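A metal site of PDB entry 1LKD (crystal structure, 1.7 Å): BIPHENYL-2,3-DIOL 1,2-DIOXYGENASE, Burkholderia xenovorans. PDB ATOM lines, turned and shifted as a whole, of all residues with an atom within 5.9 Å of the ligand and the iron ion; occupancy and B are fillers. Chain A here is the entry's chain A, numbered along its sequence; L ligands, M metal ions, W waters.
O1 of the ligand sits close to OH of Tyr 249, 2.7 Å away.
A ring nitrogen (NE2) of His 194 sits close to an oxygen (O2) of the ligand (3.3 Å).
The side-chain carboxylate of Glu 259 sits at hydrogen-bond distance from the side-chain hydroxyl of Tyr 249, 3.1 Å away.
The side-chain carboxylate (OE2) of Glu 259 sits at hydrogen-bond distance from a ring nitrogen (NE2) of His 240 (2.6 Å).
O of His 145 is in hydrogen-bond range of N of Met 211 (2.6 Å).
ND1 of His 208 is in hydrogen-bond range of ND1 of His 209 (2.7 Å).
A ring nitrogen (NE2) of His 240 sits at hydrogen-bond distance from the side-chain hydroxyl of Tyr 249 (2.9 Å).
The backbone carbonyl oxygen (O) of Pro 279 lies within hydrogen-bond range of a ring nitrogen (ND1) of His 240, at 2.9 Å.
N of His 208 lies within hydrogen-bond range of O of Val 147, 3.0 Å away.
O of Ile 172 is in hydrogen-bond range of N of Ala 184, at 2.8 Å.
Merely in contact with the ligand: Asn 242 (3.3 Å), His 240 (3.3 Å), Val 147 (3.4 Å), Phe 186 (3.5 Å), Met 174 (3.5 Å), Phe 201 (3.7 Å), Pro 279 (3.7 Å) and Ile 172 (3.8 Å).
Hydrophobic or aromatic side chains within 4 Å of the ligand: His 145, Val 147, Ile 172, Met 174, Phe 186, His 194, Phe 201, His 209, His 240, Tyr 249 and Pro 279.
The nearest printed residue that does not touch the ligand is His 208 (4.01 Å).
OH of Tyr 249 touches the iron ion, at 3.8 Å.
Four residues have an atom within 4 Å of the iron ion: His 145, His 209, Tyr 249 and Glu 259.
The nearest printed residue that does not touch the iron ion is His 194 (4.1 Å).
The iron ion is bound by O1 of the ligand (2.1 Å).
OE1 of Glu 259 binds the iron ion (2.1 Å).
O2 of the ligand binds the iron ion, 2.3 Å away.
NE2 of His 145 is bound to the iron ion.
NE2 of His 209 binds the iron ion (2.3 Å).
The iron ion is bound by water W1 (2.4 Å).
The iron ion has six donor atoms within binding distance.
Water W2 bridges OD2 of Asp 243 (2.7 Å) and OE2 of Glu 259 (3.3 Å).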
ATOM      1  N   HIS A 145      27.857  23.248  36.647  1.00  0.00           N
ATOM      2  CA  HIS A 145      27.382  21.901  36.343  1.00  0.00           C
ATOM      3  C   HIS A 145      28.484  21.014  35.791  1.00  0.00           C
ATOM      4  O   HIS A 145      29.580  21.473  35.493  1.00  0.00           O
ATOM      5  CB  HIS A 145      26.210  21.933  35.334  1.00  0.00           C
ATOM      6  CG  HIS A 145      26.605  22.263  33.923  1.00  0.00           C
ATOM      7  ND1 HIS A 145      26.252  23.440  33.299  1.00  0.00           N
ATOM      8  CD2 HIS A 145      27.282  21.541  32.989  1.00  0.00           C
ATOM      9  CE1 HIS A 145      26.688  23.435  32.054  1.00  0.00           C
ATOM     10  NE2 HIS A 145      27.322  22.298  31.846  1.00  0.00           N
ATOM     11  N   VAL A 147      28.843  17.030  33.452  1.00  0.00           N
ATOM     12  CA  VAL A 147      28.139  15.998  32.713  1.00  0.00           C
ATOM     13  C   VAL A 147      28.691  14.632  33.084  1.00  0.00           C
ATOM     14  O   VAL A 147      29.840  14.313  32.793  1.00  0.00           O
ATOM     15  CB  VAL A 147      28.306  16.236  31.206  1.00  0.00           C
ATOM     16  CG1 VAL A 147      27.496  15.198  30.431  1.00  0.00           C
ATOM     17  CG2 VAL A 147      27.863  17.642  30.864  1.00  0.00           C
ATOM     18  N   ILE A 172      18.308  16.201  24.921  1.00  0.00           N
ATOM     19  CA  ILE A 172      18.870  16.498  23.618  1.00  0.00           C
ATOM     20  C   ILE A 172      19.361  15.176  23.051  1.00  0.00           C
ATOM     21  O   ILE A 172      20.168  14.490  23.660  1.00  0.00           O
ATOM     22  CB  ILE A 172      20.065  17.476  23.693  1.00  0.00           C
ATOM     23  CG1 ILE A 172      19.599  18.826  24.243  1.00  0.00           C
ATOM     24  CG2 ILE A 172      20.656  17.676  22.302  1.00  0.00           C
ATOM     25  CD1 ILE A 172      20.726  19.835  24.431  1.00  0.00           C
ATOM     26  N   MET A 174      21.655  13.633  20.985  1.00  0.00           N
ATOM     27  CA  MET A 174      22.950  13.914  20.385  1.00  0.00           C
ATOM     28  C   MET A 174      23.308  12.992  19.234  1.00  0.00           C
ATOM     29  O   MET A 174      23.438  11.787  19.427  1.00  0.00           O
ATOM     30  CB  MET A 174      24.040  13.802  21.450  1.00  0.00           C
ATOM     31  CG  MET A 174      23.793  14.626  22.698  1.00  0.00           C
ATOM     32  SD  MET A 174      24.195  16.354  22.480  1.00  0.00           S
ATOM     33  CE  MET A 174      24.632  16.806  24.154  1.00  0.00           C
ATOM     34  N   ALA A 184      20.887  12.924  25.902  1.00  0.00           N
ATOM     35  CA  ALA A 184      21.573  13.588  26.995  1.00  0.00           C
ATOM     36  C   ALA A 184      20.451  14.216  27.824  1.00  0.00           C
ATOM     37  O   ALA A 184      19.595  14.911  27.281  1.00  0.00           O
ATOM     38  CB  ALA A 184      22.521  14.666  26.464  1.00  0.00           C
ATOM     39  N   PHE A 186      19.293  16.725  30.928  1.00  0.00           N
ATOM     40  CA  PHE A 186      19.747  17.877  31.700  1.00  0.00           C
ATOM     41  C   PHE A 186      18.818  18.041  32.884  1.00  0.00           C
ATOM     42  O   PHE A 186      17.604  18.171  32.714  1.00  0.00           O
ATOM     43  CB  PHE A 186      19.768  19.114  30.799  1.00  0.00           C
ATOM     44  CG  PHE A 186      20.698  18.959  29.633  1.00  0.00           C
ATOM     45  CD1 PHE A 186      20.332  18.170  28.538  1.00  0.00           C
ATOM     46  CD2 PHE A 186      21.956  19.525  29.653  1.00  0.00           C
ATOM     47  CE1 PHE A 186      21.221  17.952  27.495  1.00  0.00           C
ATOM     48  CE2 PHE A 186      22.858  19.312  28.607  1.00  0.00           C
ATOM     49  CZ  PHE A 186      22.488  18.519  27.526  1.00  0.00           C
ATOM     50  N   HIS A 194      20.593  23.575  34.405  1.00  0.00           N
ATOM     51  CA  HIS A 194      21.002  22.240  34.803  1.00  0.00           C
ATOM     52  C   HIS A 194      22.255  22.308  35.656  1.00  0.00           C
ATOM     53  O   HIS A 194      23.130  23.141  35.432  1.00  0.00           O
ATOM     54  CB  HIS A 194      21.192  21.260  33.602  1.00  0.00           C
ATOM     55  CG  HIS A 194      22.282  21.644  32.649  1.00  0.00           C
ATOM     56  ND1 HIS A 194      22.126  22.634  31.703  1.00  0.00           N
ATOM     57  CD2 HIS A 194      23.509  21.111  32.438  1.00  0.00           C
ATOM     58  CE1 HIS A 194      23.216  22.699  30.954  1.00  0.00           C
ATOM     59  NE2 HIS A 194      24.067  21.786  31.382  1.00  0.00           N
ATOM     60  N   ALA A 197      24.120  16.827  34.021  1.00  0.00           N
ATOM     61  CA  ALA A 197      23.653  16.276  32.758  1.00  0.00           C
ATOM     62  C   ALA A 197      24.109  14.822  32.787  1.00  0.00           C
ATOM     63  O   ALA A 197      25.109  14.496  33.415  1.00  0.00           O
ATOM     64  CB  ALA A 197      24.265  17.017  31.576  1.00  0.00           C
ATOM     65  N   PHE A 201      28.152   8.472  26.772  1.00  0.00           N
ATOM     66  CA  PHE A 201      29.160   8.797  25.774  1.00  0.00           C
ATOM     67  C   PHE A 201      30.322   7.806  25.842  1.00  0.00           C
ATOM     68  O   PHE A 201      30.582   7.231  26.898  1.00  0.00           O
ATOM     69  CB  PHE A 201      29.733  10.198  25.989  1.00  0.00           C
ATOM     70  CG  PHE A 201      28.729  11.311  25.829  1.00  0.00           C
ATOM     71  CD1 PHE A 201      27.768  11.271  24.821  1.00  0.00           C
ATOM     72  CD2 PHE A 201      28.769  12.423  26.670  1.00  0.00           C
ATOM     73  CE1 PHE A 201      26.872  12.323  24.640  1.00  0.00           C
ATOM     74  CE2 PHE A 201      27.865  13.482  26.496  1.00  0.00           C
ATOM     75  CZ  PHE A 201      26.921  13.431  25.482  1.00  0.00           C
ATOM     76  N   HIS A 208      32.342  14.348  31.189  1.00  0.00           N
ATOM     77  CA  HIS A 208      32.803  14.862  29.906  1.00  0.00           C
ATOM     78  C   HIS A 208      33.428  16.227  30.192  1.00  0.00           C
ATOM     79  O   HIS A 208      34.506  16.543  29.699  1.00  0.00           O
ATOM     80  CB  HIS A 208      31.622  14.993  28.938  1.00  0.00           C
ATOM     81  CG  HIS A 208      31.967  15.681  27.653  1.00  0.00           C
ATOM     82  ND1 HIS A 208      31.959  17.054  27.515  1.00  0.00           N
ATOM     83  CD2 HIS A 208      32.356  15.185  26.456  1.00  0.00           C
ATOM     84  CE1 HIS A 208      32.325  17.373  26.291  1.00  0.00           C
ATOM     85  NE2 HIS A 208      32.574  16.258  25.625  1.00  0.00           N
ATOM     86  N   HIS A 209      32.737  17.033  30.995  1.00  0.00           N
ATOM     87  CA  HIS A 209      33.245  18.348  31.359  1.00  0.00           C
ATOM     88  C   HIS A 209      32.517  18.899  32.572  1.00  0.00           C
ATOM     89  O   HIS A 209      31.487  18.368  32.979  1.00  0.00           O
ATOM     90  CB  HIS A 209      33.049  19.360  30.213  1.00  0.00           C
ATOM     91  CG  HIS A 209      31.618  19.700  29.929  1.00  0.00           C
ATOM     92  ND1 HIS A 209      30.823  18.955  29.096  1.00  0.00           N
ATOM     93  CD2 HIS A 209      30.854  20.741  30.350  1.00  0.00           C
ATOM     94  CE1 HIS A 209      29.623  19.509  29.003  1.00  0.00           C
ATOM     95  NE2 HIS A 209      29.612  20.598  29.758  1.00  0.00           N
ATOM     96  N   MET A 211      31.389  22.850  34.178  1.00  0.00           N
ATOM     97  CA  MET A 211      31.171  24.180  33.637  1.00  0.00           C
ATOM     98  C   MET A 211      31.194  25.271  34.702  1.00  0.00           C
ATOM     99  O   MET A 211      30.677  25.079  35.804  1.00  0.00           O
ATOM    100  CB  MET A 211      29.820  24.211  32.908  1.00  0.00           C
ATOM    101  CG  MET A 211      29.461  25.502  32.171  1.00  0.00           C
ATOM    102  SD  MET A 211      28.850  26.865  33.194  1.00  0.00           S
ATOM    103  CE  MET A 211      27.403  26.196  33.875  1.00  0.00           C
ATOM    104  N   HIS A 240      24.051  27.479  23.466  1.00  0.00           N
ATOM    105  CA  HIS A 240      23.275  26.245  23.550  1.00  0.00           C
ATOM    106  C   HIS A 240      21.795  26.436  23.287  1.00  0.00           C
ATOM    107  O   HIS A 240      21.229  27.492  23.565  1.00  0.00           O
ATOM    108  CB  HIS A 240      23.457  25.605  24.924  1.00  0.00           C
ATOM    109  CG  HIS A 240      24.811  25.017  25.136  1.00  0.00           C
ATOM    110  ND1 HIS A 240      25.310  24.002  24.348  1.00  0.00           N
ATOM    111  CD2 HIS A 240      25.769  25.295  26.058  1.00  0.00           C
ATOM    112  CE1 HIS A 240      26.513  23.682  24.771  1.00  0.00           C
ATOM    113  NE2 HIS A 240      26.816  24.453  25.800  1.00  0.00           N
ATOM    114  N   THR A 241      21.170  25.399  22.746  1.00  0.00           N
ATOM    115  CA  THR A 241      19.742  25.431  22.437  1.00  0.00           C
ATOM    116  C   THR A 241      18.868  25.367  23.676  1.00  0.00           C
ATOM    117  O   THR A 241      17.781  25.948  23.709  1.00  0.00           O
ATOM    118  CB  THR A 241      19.362  24.237  21.557  1.00  0.00           C
ATOM    119  OG1 THR A 241      19.862  23.041  22.160  1.00  0.00           O
ATOM    120  CG2 THR A 241      19.936  24.392  20.157  1.00  0.00           C
ATOM    121  N   ASN A 242      19.325  24.653  24.712  1.00  0.00           N
ATOM    122  CA  ASN A 242      18.496  24.490  25.897  1.00  0.00           C
ATOM    123  C   ASN A 242      18.664  25.524  27.004  1.00  0.00           C
ATOM    124  O   ASN A 242      17.673  26.101  27.436  1.00  0.00           O
ATOM    125  CB  ASN A 242      18.630  23.063  26.458  1.00  0.00           C
ATOM    126  CG  ASN A 242      20.060  22.665  26.817  1.00  0.00           C
ATOM    127  OD1 ASN A 242      21.016  23.376  26.526  1.00  0.00           O
ATOM    128  ND2 ASN A 242      20.194  21.511  27.455  1.00  0.00           N
ATOM    129  N   ASP A 243      19.890  25.775  27.464  1.00  0.00           N
ATOM    130  CA  ASP A 243      20.051  26.770  28.513  1.00  0.00           C
ATOM    131  C   ASP A 243      20.454  28.136  27.960  1.00  0.00           C
ATOM    132  O   ASP A 243      20.565  29.096  28.716  1.00  0.00           O
ATOM    133  CB  ASP A 243      21.048  26.281  29.571  1.00  0.00           C
ATOM    134  CG  ASP A 243      22.481  26.320  29.094  1.00  0.00           C
ATOM    135  OD1 ASP A 243      22.720  26.458  27.879  1.00  0.00           O
ATOM    136  OD2 ASP A 243      23.379  26.209  29.969  1.00  0.00           O
ATOM    137  N   TYR A 249      34.506  25.441  24.848  1.00  0.00           N
ATOM    138  CA  TYR A 249      35.022  24.309  25.608  1.00  0.00           C
ATOM    139  C   TYR A 249      36.531  24.228  25.411  1.00  0.00           C
ATOM    140  O   TYR A 249      37.058  24.636  24.379  1.00  0.00           O
ATOM    141  CB  TYR A 249      34.397  22.993  25.140  1.00  0.00           C
ATOM    142  CG  TYR A 249      32.914  22.886  25.396  1.00  0.00           C
ATOM    143  CD1 TYR A 249      31.983  23.547  24.584  1.00  0.00           C
ATOM    144  CD2 TYR A 249      32.426  22.074  26.415  1.00  0.00           C
ATOM    145  CE1 TYR A 249      30.619  23.394  24.789  1.00  0.00           C
ATOM    146  CE2 TYR A 249      31.058  21.918  26.633  1.00  0.00           C
ATOM    147  CZ  TYR A 249      30.163  22.584  25.816  1.00  0.00           C
ATOM    148  OH  TYR A 249      28.821  22.399  26.002  1.00  0.00           O
ATOM    149  N   GLU A 259      33.844  23.809  30.400  1.00  0.00           N
ATOM    150  CA  GLU A 259      33.012  24.704  29.610  1.00  0.00           C
ATOM    151  C   GLU A 259      33.033  26.021  30.382  1.00  0.00           C
ATOM    152  O   GLU A 259      32.905  26.031  31.606  1.00  0.00           O
ATOM    153  CB  GLU A 259      31.597  24.172  29.492  1.00  0.00           C
ATOM    154  CG  GLU A 259      30.678  25.106  28.744  1.00  0.00           C
ATOM    155  CD  GLU A 259      29.294  24.543  28.550  1.00  0.00           C
ATOM    156  OE1 GLU A 259      28.914  23.607  29.289  1.00  0.00           O
ATOM    157  OE2 GLU A 259      28.561  25.046  27.659  1.00  0.00           O
ATOM    158  N   PRO A 279      22.471  20.482  20.113  1.00  0.00           N
ATOM    159  CA  PRO A 279      22.847  21.083  21.391  1.00  0.00           C
ATOM    160  C   PRO A 279      23.236  22.560  21.265  1.00  0.00           C
ATOM    161  O   PRO A 279      23.380  23.249  22.278  1.00  0.00           O
ATOM    162  CB  PRO A 279      24.021  20.226  21.838  1.00  0.00           C
ATOM    163  CG  PRO A 279      24.733  19.994  20.544  1.00  0.00           C
ATOM    164  CD  PRO A 279      23.593  19.678  19.574  1.00  0.00           C
ATOM    165  N   SER A 280      23.402  23.034  20.043  1.00  0.00           N
ATOM    166  CA  SER A 280      23.814  24.426  19.824  1.00  0.00           C
ATOM    167  C   SER A 280      22.999  25.189  18.775  1.00  0.00           C
ATOM    168  O   SER A 280      22.751  24.676  17.681  1.00  0.00           O
ATOM    169  CB  SER A 280      25.289  24.462  19.425  1.00  0.00           C
ATOM    170  OG  SER A 280      26.089  23.798  20.393  1.00  0.00           O
ATOM    171  N   HIS A 284      29.977  26.613  18.509  1.00  0.00           N
ATOM    172  CA  HIS A 284      30.365  25.360  19.136  1.00  0.00           C
ATOM    173  C   HIS A 284      30.868  24.375  18.087  1.00  0.00           C
ATOM    174  O   HIS A 284      30.549  23.180  18.112  1.00  0.00           O
ATOM    175  CB  HIS A 284      29.202  24.756  19.913  1.00  0.00           C
ATOM    176  CG  HIS A 284      28.929  25.451  21.217  1.00  0.00           C
ATOM    177  ND1 HIS A 284      27.688  25.470  21.809  1.00  0.00           N
ATOM    178  CD2 HIS A 284      29.754  26.131  22.047  1.00  0.00           C
ATOM    179  CE1 HIS A 284      27.759  26.129  22.954  1.00  0.00           C
ATOM    180  NE2 HIS A 284      29.003  26.545  23.118  1.00  0.00           N
HETATM  181  C1  LIG L   1      25.837  20.339  26.107  1.00  0.00           C
HETATM  182  C2  LIG L   1      26.207  21.140  27.207  1.00  0.00           C
HETATM  183  O1  LIG L   1      27.423  21.000  27.819  1.00  0.00           O
HETATM  184  C3  LIG L   1      25.351  22.124  27.740  1.00  0.00           C
HETATM  185  O2  LIG L   1      25.801  22.847  28.829  1.00  0.00           O
HETATM  186  C4  LIG L   1      24.069  22.324  27.158  1.00  0.00           C
HETATM  187  C5  LIG L   1      23.683  21.533  26.043  1.00  0.00           C
HETATM  188  C6  LIG L   1      24.567  20.543  25.522  1.00  0.00           C
HETATM  189  C7  LIG L   1      26.809  19.299  25.594  1.00  0.00           C
HETATM  190  C8  LIG L   1      27.043  18.109  26.345  1.00  0.00           C
HETATM  191  C9  LIG L   1      27.961  17.119  25.900  1.00  0.00           C
HETATM  192  C10 LIG L   1      28.657  17.291  24.685  1.00  0.00           C
HETATM  193  C11 LIG L   1      28.437  18.457  23.924  1.00  0.00           C
HETATM  194  C12 LIG L   1      27.519  19.447  24.368  1.00  0.00           C
HETATM  195 CL1  LIG L   1      26.255  17.725  27.862  1.00  0.00          CL
HETATM  196 CL2  LIG L   1      27.376  20.812  23.289  1.00  0.00          CL
HETATM  197 FE    FE M   1      27.742  21.942  29.624  1.00  0.00          FE
HETATM  198  O   HOH W   1      26.234  20.151  30.233  1.00  0.00           O
HETATM  199  O   HOH W   2      25.963  25.629  29.677  1.00  0.00           O
